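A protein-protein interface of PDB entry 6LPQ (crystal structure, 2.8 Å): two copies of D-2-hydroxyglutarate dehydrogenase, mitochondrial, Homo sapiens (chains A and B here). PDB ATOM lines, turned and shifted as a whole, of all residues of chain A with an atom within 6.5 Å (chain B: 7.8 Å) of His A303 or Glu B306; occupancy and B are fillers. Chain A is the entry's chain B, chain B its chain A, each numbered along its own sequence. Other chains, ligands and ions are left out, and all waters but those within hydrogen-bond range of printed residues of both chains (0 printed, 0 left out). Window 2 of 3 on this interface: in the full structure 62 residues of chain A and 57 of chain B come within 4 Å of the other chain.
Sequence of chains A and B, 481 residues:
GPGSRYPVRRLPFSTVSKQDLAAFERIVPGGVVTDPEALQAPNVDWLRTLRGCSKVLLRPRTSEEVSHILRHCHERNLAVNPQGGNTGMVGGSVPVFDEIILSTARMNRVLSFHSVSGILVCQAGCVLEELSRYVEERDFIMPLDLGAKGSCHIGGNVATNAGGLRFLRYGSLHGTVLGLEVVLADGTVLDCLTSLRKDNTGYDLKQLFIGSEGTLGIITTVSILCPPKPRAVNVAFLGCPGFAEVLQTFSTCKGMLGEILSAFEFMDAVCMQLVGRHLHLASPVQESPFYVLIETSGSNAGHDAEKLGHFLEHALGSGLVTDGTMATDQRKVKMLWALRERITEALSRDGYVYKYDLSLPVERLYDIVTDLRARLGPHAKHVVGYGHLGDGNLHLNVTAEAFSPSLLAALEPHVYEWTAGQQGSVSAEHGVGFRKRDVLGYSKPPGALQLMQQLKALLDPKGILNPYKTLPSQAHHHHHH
OE2 of Glu B259 lies within salt-bridge range of NZ of Lys B307, at 3.9 Å. ND1 of His B303 lies within hydrogen-bond range of OD1 of Asn B300 (2.7 Å). N of Gly A302 lies within hydrogen-bond range of OD1 of Asn A300 (3.2 Å). The side-chain amide oxygen (OD1) of Asn A300 is in hydrogen-bond range of the backbone NH (N) of His A303.
Asn A300 touches Lys B307, but with the chains exchanged Lys A307 does not touch Asn B300 (4.8 Å). His A303 touches its own counterpart, His B303. His A303 touches Glu B306, and with the chains exchanged Glu A306 touches His B303. His A303 touches Lys B307, and with the chains exchanged Lys A307 touches His B303.
Of the printed residues of chain B, Asn A300 touches Lys B307 (3.9 Å). No residue of chain B comes within 4 Å of Gly A302. Of the printed residues of chain B, His A303 touches His B303 (3.5 Å), Glu B306 (3.999 Å) and Lys B307 (3.0 Å). Printed residues of chain B within 4 Å of Lys A307: His B303 (3.7 Å). Met B256 touches none of the printed residues of chain A. Of the printed residues of chain A, Glu B259 touches Ile A260 (3.96 Å). Of the printed residues of chain A, His B303 touches His A303 (3.5 Å), Glu A306 (3.1 Å) and Lys A307 (3.7 Å). Ala B305 touches none of the printed residues of chain A. Of the printed residues of chain A, Glu B306 touches His A303. Printed residues of chain A within 4 Å of Lys B307: Asn A300 (3.9 Å) and His A303 (3.0 Å).
Ile A260 touches Glu B259. CB of Asn A300 touches CE of Lys B307, 3.9 Å away. His A303 touches His B303. NE2 of His A303 touches CB of Glu B306, 3.999 Å away. Lys A307 touches His B303 (CG to CE1, 3.7 Å).
NE2 of His B303 sits at hydrogen-bond distance from OE1 of Glu A306, 3.1 Å away. The side-chain amino group (NZ) of Lys B307 is in hydrogen-bond range of a ring nitrogen (ND1) of His A303 (3.0 Å).
Printed residues of chain A that touch a printed residue of chain B: Ile A260, Asn A300, His A303, Glu A306 and Lys A307. Hydrophobic or aromatic side chains of chain A within 4 Å of the printed part of chain B: Ile A260 and His A303. Among the printed residues, no Asp or Glu carboxylate lies within 4 Å of a Lys or Arg side-chain nitrogen of the other chain.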
ATOM      1  N   ILE A 260     -23.525  -5.139   3.040  1.00  0.00           N
ATOM      2  CA  ILE A 260     -23.667  -4.158   4.118  1.00  0.00           C
ATOM      3  C   ILE A 260     -22.846  -2.893   3.906  1.00  0.00           C
ATOM      4  O   ILE A 260     -23.049  -1.915   4.636  1.00  0.00           O
ATOM      5  CB  ILE A 260     -23.309  -4.773   5.484  1.00  0.00           C
ATOM      6  CG1 ILE A 260     -21.803  -5.021   5.589  1.00  0.00           C
ATOM      7  CG2 ILE A 260     -24.112  -6.038   5.724  1.00  0.00           C
ATOM      8  CD1 ILE A 260     -21.334  -5.341   6.988  1.00  0.00           C
ATOM      9  N   ASN A 300     -28.634  -6.542  11.107  1.00  0.00           N
ATOM     10  CA  ASN A 300     -28.229  -7.286  12.296  1.00  0.00           C
ATOM     11  C   ASN A 300     -26.869  -6.789  12.768  1.00  0.00           C
ATOM     12  O   ASN A 300     -25.852  -7.020  12.104  1.00  0.00           O
ATOM     13  CB  ASN A 300     -28.180  -8.784  12.003  1.00  0.00           C
ATOM     14  CG  ASN A 300     -28.165  -9.623  13.258  1.00  0.00           C
ATOM     15  OD1 ASN A 300     -27.160  -9.681  13.968  1.00  0.00           O
ATOM     16  ND2 ASN A 300     -29.277 -10.287  13.537  1.00  0.00           N
ATOM     17  N   ALA A 301     -26.863  -6.102  13.913  1.00  0.00           N
ATOM     18  CA  ALA A 301     -25.629  -5.573  14.488  1.00  0.00           C
ATOM     19  C   ALA A 301     -24.573  -6.658  14.662  1.00  0.00           C
ATOM     20  O   ALA A 301     -23.430  -6.510  14.214  1.00  0.00           O
ATOM     21  CB  ALA A 301     -25.925  -4.896  15.827  1.00  0.00           C
ATOM     22  N   GLY A 302     -24.947  -7.753  15.330  1.00  0.00           N
ATOM     23  CA  GLY A 302     -24.037  -8.878  15.511  1.00  0.00           C
ATOM     24  C   GLY A 302     -23.404  -9.387  14.231  1.00  0.00           C
ATOM     25  O   GLY A 302     -22.191  -9.606  14.171  1.00  0.00           O
ATOM     26  N   HIS A 303     -24.209  -9.575  13.183  1.00  0.00           N
ATOM     27  CA  HIS A 303     -23.660 -10.057  11.918  1.00  0.00           C
ATOM     28  C   HIS A 303     -22.732  -9.030  11.279  1.00  0.00           C
ATOM     29  O   HIS A 303     -21.652  -9.385  10.790  1.00  0.00           O
ATOM     30  CB  HIS A 303     -24.786 -10.436  10.957  1.00  0.00           C
ATOM     31  CG  HIS A 303     -25.640 -11.564  11.444  1.00  0.00           C
ATOM     32  ND1 HIS A 303     -26.928 -11.772  10.999  1.00  0.00           N
ATOM     33  CD2 HIS A 303     -25.391 -12.543  12.346  1.00  0.00           C
ATOM     34  CE1 HIS A 303     -27.433 -12.836  11.599  1.00  0.00           C
ATOM     35  NE2 HIS A 303     -26.521 -13.320  12.422  1.00  0.00           N
ATOM     36  N   ASP A 304     -23.127  -7.758  11.281  1.00  0.00           N
ATOM     37  CA  ASP A 304     -22.271  -6.713  10.728  1.00  0.00           C
ATOM     38  C   ASP A 304     -20.964  -6.600  11.500  1.00  0.00           C
ATOM     39  O   ASP A 304     -19.899  -6.398  10.905  1.00  0.00           O
ATOM     40  CB  ASP A 304     -23.011  -5.378  10.726  1.00  0.00           C
ATOM     41  CG  ASP A 304     -24.183  -5.364   9.769  1.00  0.00           C
ATOM     42  OD1 ASP A 304     -24.520  -6.433   9.215  1.00  0.00           O
ATOM     43  OD2 ASP A 304     -24.768  -4.282   9.568  1.00  0.00           O
ATOM     44  N   ALA A 305     -21.027  -6.724  12.826  1.00  0.00           N
ATOM     45  CA  ALA A 305     -19.814  -6.702  13.636  1.00  0.00           C
ATOM     46  C   ALA A 305     -18.885  -7.863  13.300  1.00  0.00           C
ATOM     47  O   ALA A 305     -17.667  -7.675  13.191  1.00  0.00           O
ATOM     48  CB  ALA A 305     -20.176  -6.722  15.121  1.00  0.00           C
ATOM     49  N   GLU A 306     -19.431  -9.071  13.137  1.00  0.00           N
ATOM     50  CA  GLU A 306     -18.598 -10.203  12.738  1.00  0.00           C
ATOM     51  C   GLU A 306     -17.945  -9.978  11.378  1.00  0.00           C
ATOM     52  O   GLU A 306     -16.742 -10.211  11.213  1.00  0.00           O
ATOM     53  CB  GLU A 306     -19.433 -11.486  12.706  1.00  0.00           C
ATOM     54  CG  GLU A 306     -19.264 -12.401  13.908  1.00  0.00           C
ATOM     55  CD  GLU A 306     -20.073 -13.683  13.780  1.00  0.00           C
ATOM     56  OE1 GLU A 306     -19.844 -14.444  12.814  1.00  0.00           O
ATOM     57  OE2 GLU A 306     -20.945 -13.926  14.641  1.00  0.00           O
ATOM     58  N   LYS A 307     -18.720  -9.529  10.388  1.00  0.00           N
ATOM     59  CA  LYS A 307     -18.149  -9.209   9.080  1.00  0.00           C
ATOM     60  C   LYS A 307     -17.029  -8.176   9.176  1.00  0.00           C
ATOM     61  O   LYS A 307     -15.947  -8.362   8.608  1.00  0.00           O
ATOM     62  CB  LYS A 307     -19.247  -8.741   8.123  1.00  0.00           C
ATOM     63  CG  LYS A 307     -20.052  -9.887   7.523  1.00  0.00           C
ATOM     64  CD  LYS A 307     -20.962  -9.416   6.402  1.00  0.00           C
ATOM     65  CE  LYS A 307     -22.267  -8.862   6.948  1.00  0.00           C
ATOM     66  NZ  LYS A 307     -23.430  -9.729   6.606  1.00  0.00           N
ATOM     67  N   LEU A 308     -17.279  -7.075   9.885  1.00  0.00           N
ATOM     68  CA  LEU A 308     -16.268  -6.032  10.048  1.00  0.00           C
ATOM     69  C   LEU A 308     -15.055  -6.520  10.830  1.00  0.00           C
ATOM     70  O   LEU A 308     -13.912  -6.221  10.462  1.00  0.00           O
ATOM     71  CB  LEU A 308     -16.894  -4.815  10.720  1.00  0.00           C
ATOM     72  CG  LEU A 308     -17.437  -3.833   9.689  1.00  0.00           C
ATOM     73  CD1 LEU A 308     -18.531  -3.007  10.300  1.00  0.00           C
ATOM     74  CD2 LEU A 308     -16.319  -2.942   9.168  1.00  0.00           C
ATOM     75  N   ASN B 234     -30.581 -18.052  -1.226  1.00  0.00           N
ATOM     76  CA  ASN B 234     -31.590 -18.875  -0.584  1.00  0.00           C
ATOM     77  C   ASN B 234     -32.971 -18.502  -1.100  1.00  0.00           C
ATOM     78  O   ASN B 234     -33.234 -17.346  -1.443  1.00  0.00           O
ATOM     79  CB  ASN B 234     -31.543 -18.704   0.936  1.00  0.00           C
ATOM     80  CG  ASN B 234     -30.261 -19.233   1.537  1.00  0.00           C
ATOM     81  OD1 ASN B 234     -30.147 -20.414   1.862  1.00  0.00           O
ATOM     82  ND2 ASN B 234     -29.280 -18.354   1.685  1.00  0.00           N
ATOM     83  N   MET B 256     -36.546  -8.429   9.228  1.00  0.00           N
ATOM     84  CA  MET B 256     -35.671  -9.487   9.720  1.00  0.00           C
ATOM     85  C   MET B 256     -34.619  -9.938   8.719  1.00  0.00           C
ATOM     86  O   MET B 256     -33.573 -10.443   9.134  1.00  0.00           O
ATOM     87  CB  MET B 256     -36.494 -10.699  10.166  1.00  0.00           C
ATOM     88  CG  MET B 256     -37.467 -10.397  11.298  1.00  0.00           C
ATOM     89  SD  MET B 256     -38.207 -11.883  11.994  1.00  0.00           S
ATOM     90  CE  MET B 256     -36.844 -12.524  12.965  1.00  0.00           C
ATOM     91  N   LEU B 257     -34.858  -9.774   7.421  1.00  0.00           N
ATOM     92  CA  LEU B 257     -33.862 -10.119   6.414  1.00  0.00           C
ATOM     93  C   LEU B 257     -33.139  -8.891   5.883  1.00  0.00           C
ATOM     94  O   LEU B 257     -31.923  -8.932   5.681  1.00  0.00           O
ATOM     95  CB  LEU B 257     -34.513 -10.877   5.253  1.00  0.00           C
ATOM     96  CG  LEU B 257     -35.254 -12.164   5.628  1.00  0.00           C
ATOM     97  CD1 LEU B 257     -35.805 -12.854   4.389  1.00  0.00           C
ATOM     98  CD2 LEU B 257     -34.359 -13.104   6.421  1.00  0.00           C
ATOM     99  N   GLU B 259     -31.197  -6.086   4.133  1.00  0.00           N
ATOM    100  CA  GLU B 259     -30.370  -5.848   2.953  1.00  0.00           C
ATOM    101  C   GLU B 259     -30.068  -7.099   2.137  1.00  0.00           C
ATOM    102  O   GLU B 259     -29.671  -6.971   0.974  1.00  0.00           O
ATOM    103  CB  GLU B 259     -29.054  -5.170   3.354  1.00  0.00           C
ATOM    104  CG  GLU B 259     -28.065  -6.026   4.145  1.00  0.00           C
ATOM    105  CD  GLU B 259     -28.514  -6.335   5.565  1.00  0.00           C
ATOM    106  OE1 GLU B 259     -29.489  -5.719   6.045  1.00  0.00           O
ATOM    107  OE2 GLU B 259     -27.868  -7.186   6.211  1.00  0.00           O
ATOM    108  N   ILE B 260     -30.221  -8.301   2.699  1.00  0.00           N
ATOM    109  CA  ILE B 260     -29.986  -9.493   1.884  1.00  0.00           C
ATOM    110  C   ILE B 260     -31.171  -9.853   1.002  1.00  0.00           C
ATOM    111  O   ILE B 260     -31.028 -10.708   0.120  1.00  0.00           O
ATOM    112  CB  ILE B 260     -29.591 -10.696   2.762  1.00  0.00           C
ATOM    113  CG1 ILE B 260     -30.765 -11.156   3.629  1.00  0.00           C
ATOM    114  CG2 ILE B 260     -28.371 -10.364   3.611  1.00  0.00           C
ATOM    115  CD1 ILE B 260     -30.538 -12.495   4.307  1.00  0.00           C
ATOM    116  N   ASN B 300     -22.112 -13.680   3.105  1.00  0.00           N
ATOM    117  CA  ASN B 300     -21.788 -14.700   4.100  1.00  0.00           C
ATOM    118  C   ASN B 300     -22.967 -15.651   4.257  1.00  0.00           C
ATOM    119  O   ASN B 300     -24.000 -15.282   4.827  1.00  0.00           O
ATOM    120  CB  ASN B 300     -21.400 -14.082   5.439  1.00  0.00           C
ATOM    121  CG  ASN B 300     -20.904 -15.119   6.428  1.00  0.00           C
ATOM    122  OD1 ASN B 300     -21.107 -14.991   7.632  1.00  0.00           O
ATOM    123  ND2 ASN B 300     -20.267 -16.167   5.918  1.00  0.00           N
ATOM    124  N   ALA B 301     -22.801 -16.871   3.742  1.00  0.00           N
ATOM    125  CA  ALA B 301     -23.885 -17.847   3.731  1.00  0.00           C
ATOM    126  C   ALA B 301     -24.363 -18.166   5.140  1.00  0.00           C
ATOM    127  O   ALA B 301     -25.555 -18.413   5.357  1.00  0.00           O
ATOM    128  CB  ALA B 301     -23.427 -19.124   3.027  1.00  0.00           C
ATOM    129  N   GLY B 302     -23.450 -18.192   6.109  1.00  0.00           N
ATOM    130  CA  GLY B 302     -23.860 -18.494   7.469  1.00  0.00           C
ATOM    131  C   GLY B 302     -24.705 -17.401   8.096  1.00  0.00           C
ATOM    132  O   GLY B 302     -25.690 -17.692   8.777  1.00  0.00           O
ATOM    133  N   HIS B 303     -24.341 -16.132   7.877  1.00  0.00           N
ATOM    134  CA  HIS B 303     -25.170 -15.036   8.378  1.00  0.00           C
ATOM    135  C   HIS B 303     -26.556 -15.034   7.741  1.00  0.00           C
ATOM    136  O   HIS B 303     -27.562 -14.833   8.432  1.00  0.00           O
ATOM    137  CB  HIS B 303     -24.481 -13.688   8.155  1.00  0.00           C
ATOM    138  CG  HIS B 303     -23.264 -13.476   9.001  1.00  0.00           C
ATOM    139  ND1 HIS B 303     -22.189 -12.719   8.585  1.00  0.00           N
ATOM    140  CD2 HIS B 303     -22.962 -13.905  10.250  1.00  0.00           C
ATOM    141  CE1 HIS B 303     -21.273 -12.701   9.537  1.00  0.00           C
ATOM    142  NE2 HIS B 303     -21.716 -13.412  10.557  1.00  0.00           N
ATOM    143  N   ASP B 304     -26.631 -15.256   6.427  1.00  0.00           N
ATOM    144  CA  ASP B 304     -27.927 -15.328   5.756  1.00  0.00           C
ATOM    145  C   ASP B 304     -28.777 -16.464   6.309  1.00  0.00           C
ATOM    146  O   ASP B 304     -29.944 -16.264   6.667  1.00  0.00           O
ATOM    147  CB  ASP B 304     -27.730 -15.492   4.252  1.00  0.00           C
ATOM    148  CG  ASP B 304     -27.089 -14.281   3.613  1.00  0.00           C
ATOM    149  OD1 ASP B 304     -26.687 -13.350   4.346  1.00  0.00           O
ATOM    150  OD2 ASP B 304     -27.000 -14.258   2.370  1.00  0.00           O
ATOM    151  N   ALA B 305     -28.196 -17.661   6.408  1.00  0.00           N
ATOM    152  CA  ALA B 305     -28.927 -18.811   6.929  1.00  0.00           C
ATOM    153  C   ALA B 305     -29.430 -18.548   8.341  1.00  0.00           C
ATOM    154  O   ALA B 305     -30.547 -18.941   8.698  1.00  0.00           O
ATOM    155  CB  ALA B 305     -28.037 -20.052   6.901  1.00  0.00           C
ATOM    156  N   GLU B 306     -28.615 -17.881   9.155  1.00  0.00           N
ATOM    157  CA  GLU B 306     -29.039 -17.492  10.495  1.00  0.00           C
ATOM    158  C   GLU B 306     -30.213 -16.515  10.448  1.00  0.00           C
ATOM    159  O   GLU B 306     -31.165 -16.641  11.229  1.00  0.00           O
ATOM    160  CB  GLU B 306     -27.826 -16.900  11.208  1.00  0.00           C
ATOM    161  CG  GLU B 306     -26.808 -17.981  11.582  1.00  0.00           C
ATOM    162  CD  GLU B 306     -25.614 -17.460  12.357  1.00  0.00           C
ATOM    163  OE1 GLU B 306     -24.612 -17.097  11.700  1.00  0.00           O
ATOM    164  OE2 GLU B 306     -25.660 -17.422  13.603  1.00  0.00           O
ATOM    165  N   LYS B 307     -30.163 -15.533   9.544  1.00  0.00           N
ATOM    166  CA  LYS B 307     -31.277 -14.598   9.385  1.00  0.00           C
ATOM    167  C   LYS B 307     -32.553 -15.321   8.964  1.00  0.00           C
ATOM    168  O   LYS B 307     -33.633 -15.073   9.511  1.00  0.00           O
ATOM    169  CB  LYS B 307     -30.919 -13.512   8.371  1.00  0.00           C
ATOM    170  CG  LYS B 307     -30.027 -12.411   8.919  1.00  0.00           C
ATOM    171  CD  LYS B 307     -29.755 -11.358   7.856  1.00  0.00           C
ATOM    172  CE  LYS B 307     -29.044 -10.148   8.440  1.00  0.00           C
ATOM    173  NZ  LYS B 307     -27.564 -10.325   8.436  1.00  0.00           N
ATOM    174  N   LEU B 308     -32.442 -16.215   7.978  1.00  0.00           N
ATOM    175  CA  LEU B 308     -33.596 -16.985   7.520  1.00  0.00           C
ATOM    176  C   LEU B 308     -34.171 -17.866   8.623  1.00  0.00           C
ATOM    177  O   LEU B 308     -35.394 -17.952   8.780  1.00  0.00           O
ATOM    178  CB  LEU B 308     -33.214 -17.838   6.308  1.00  0.00           C
ATOM    179  CG  LEU B 308     -33.348 -17.239   4.903  1.00  0.00           C
ATOM    180  CD1 LEU B 308     -34.729 -16.631   4.701  1.00  0.00           C
ATOM    181  CD2 LEU B 308     -32.261 -16.215   4.609  1.00  0.00           C
ATOM    182  N   GLY B 309     -33.309 -18.543   9.383  1.00  0.00           N
ATOM    183  CA  GLY B 309     -33.789 -19.391  10.466  1.00  0.00           C
ATOM    184  C   GLY B 309     -34.668 -18.658  11.464  1.00  0.00           C
ATOM    185  O   GLY B 309     -35.788 -19.085  11.755  1.00  0.00           O
ATOM    186  N   HIS B 310     -34.176 -17.537  11.998  1.00  0.00           N
ATOM    187  CA  HIS B 310     -34.968 -16.774  12.959  1.00  0.00           C
ATOM    188  C   HIS B 310     -36.225 -16.198  12.316  1.00  0.00           C
ATOM    189  O   HIS B 310     -37.282 -16.148  12.955  1.00  0.00           O
ATOM    190  CB  HIS B 310     -34.115 -15.686  13.615  1.00  0.00           C
ATOM    191  CG  HIS B 310     -33.020 -16.230  14.484  1.00  0.00           C
ATOM    192  ND1 HIS B 310     -32.730 -17.575  14.561  1.00  0.00           N
ATOM    193  CD2 HIS B 310     -32.167 -15.614  15.338  1.00  0.00           C
ATOM    194  CE1 HIS B 310     -31.736 -17.763  15.411  1.00  0.00           C
ATOM    195  NE2 HIS B 310     -31.377 -16.589  15.896  1.00  0.00           N
ATOM    196  N   PHE B 311     -36.128 -15.737  11.068  1.00  0.00           N
ATOM    197  CA  PHE B 311     -37.317 -15.260  10.367  1.00  0.00           C
ATOM    198  C   PHE B 311     -38.360 -16.367  10.240  1.00  0.00           C
ATOM    199  O   PHE B 311     -39.534 -16.177  10.582  1.00  0.00           O
ATOM    200  CB  PHE B 311     -36.918 -14.733   8.987  1.00  0.00           C
ATOM    201  CG  PHE B 311     -38.083 -14.425   8.089  1.00  0.00           C
ATOM    202  CD1 PHE B 311     -38.916 -13.351   8.348  1.00  0.00           C
ATOM    203  CD2 PHE B 311     -38.339 -15.210   6.976  1.00  0.00           C
ATOM    204  CE1 PHE B 311     -39.986 -13.070   7.516  1.00  0.00           C
ATOM    205  CE2 PHE B 311     -39.407 -14.934   6.142  1.00  0.00           C
ATOM    206  CZ  PHE B 311     -40.230 -13.863   6.411  1.00  0.00           C
ATOM    207  N   LEU B 312     -37.946 -17.533   9.742  1.00  0.00           N
ATOM    208  CA  LEU B 312     -38.866 -18.653   9.558  1.00  0.00           C
ATOM    209  C   LEU B 312     -39.500 -19.131  10.862  1.00  0.00           C
ATOM    210  O   LEU B 312     -40.721 -19.310  10.936  1.00  0.00           O
ATOM    211  CB  LEU B 312     -38.140 -19.815   8.881  1.00  0.00           C
ATOM    212  CG  LEU B 312     -39.034 -20.879   8.239  1.00  0.00           C
ATOM    213  CD1 LEU B 312     -40.148 -20.261   7.408  1.00  0.00           C
ATOM    214  CD2 LEU B 312     -38.215 -21.855   7.409  1.00  0.00           C
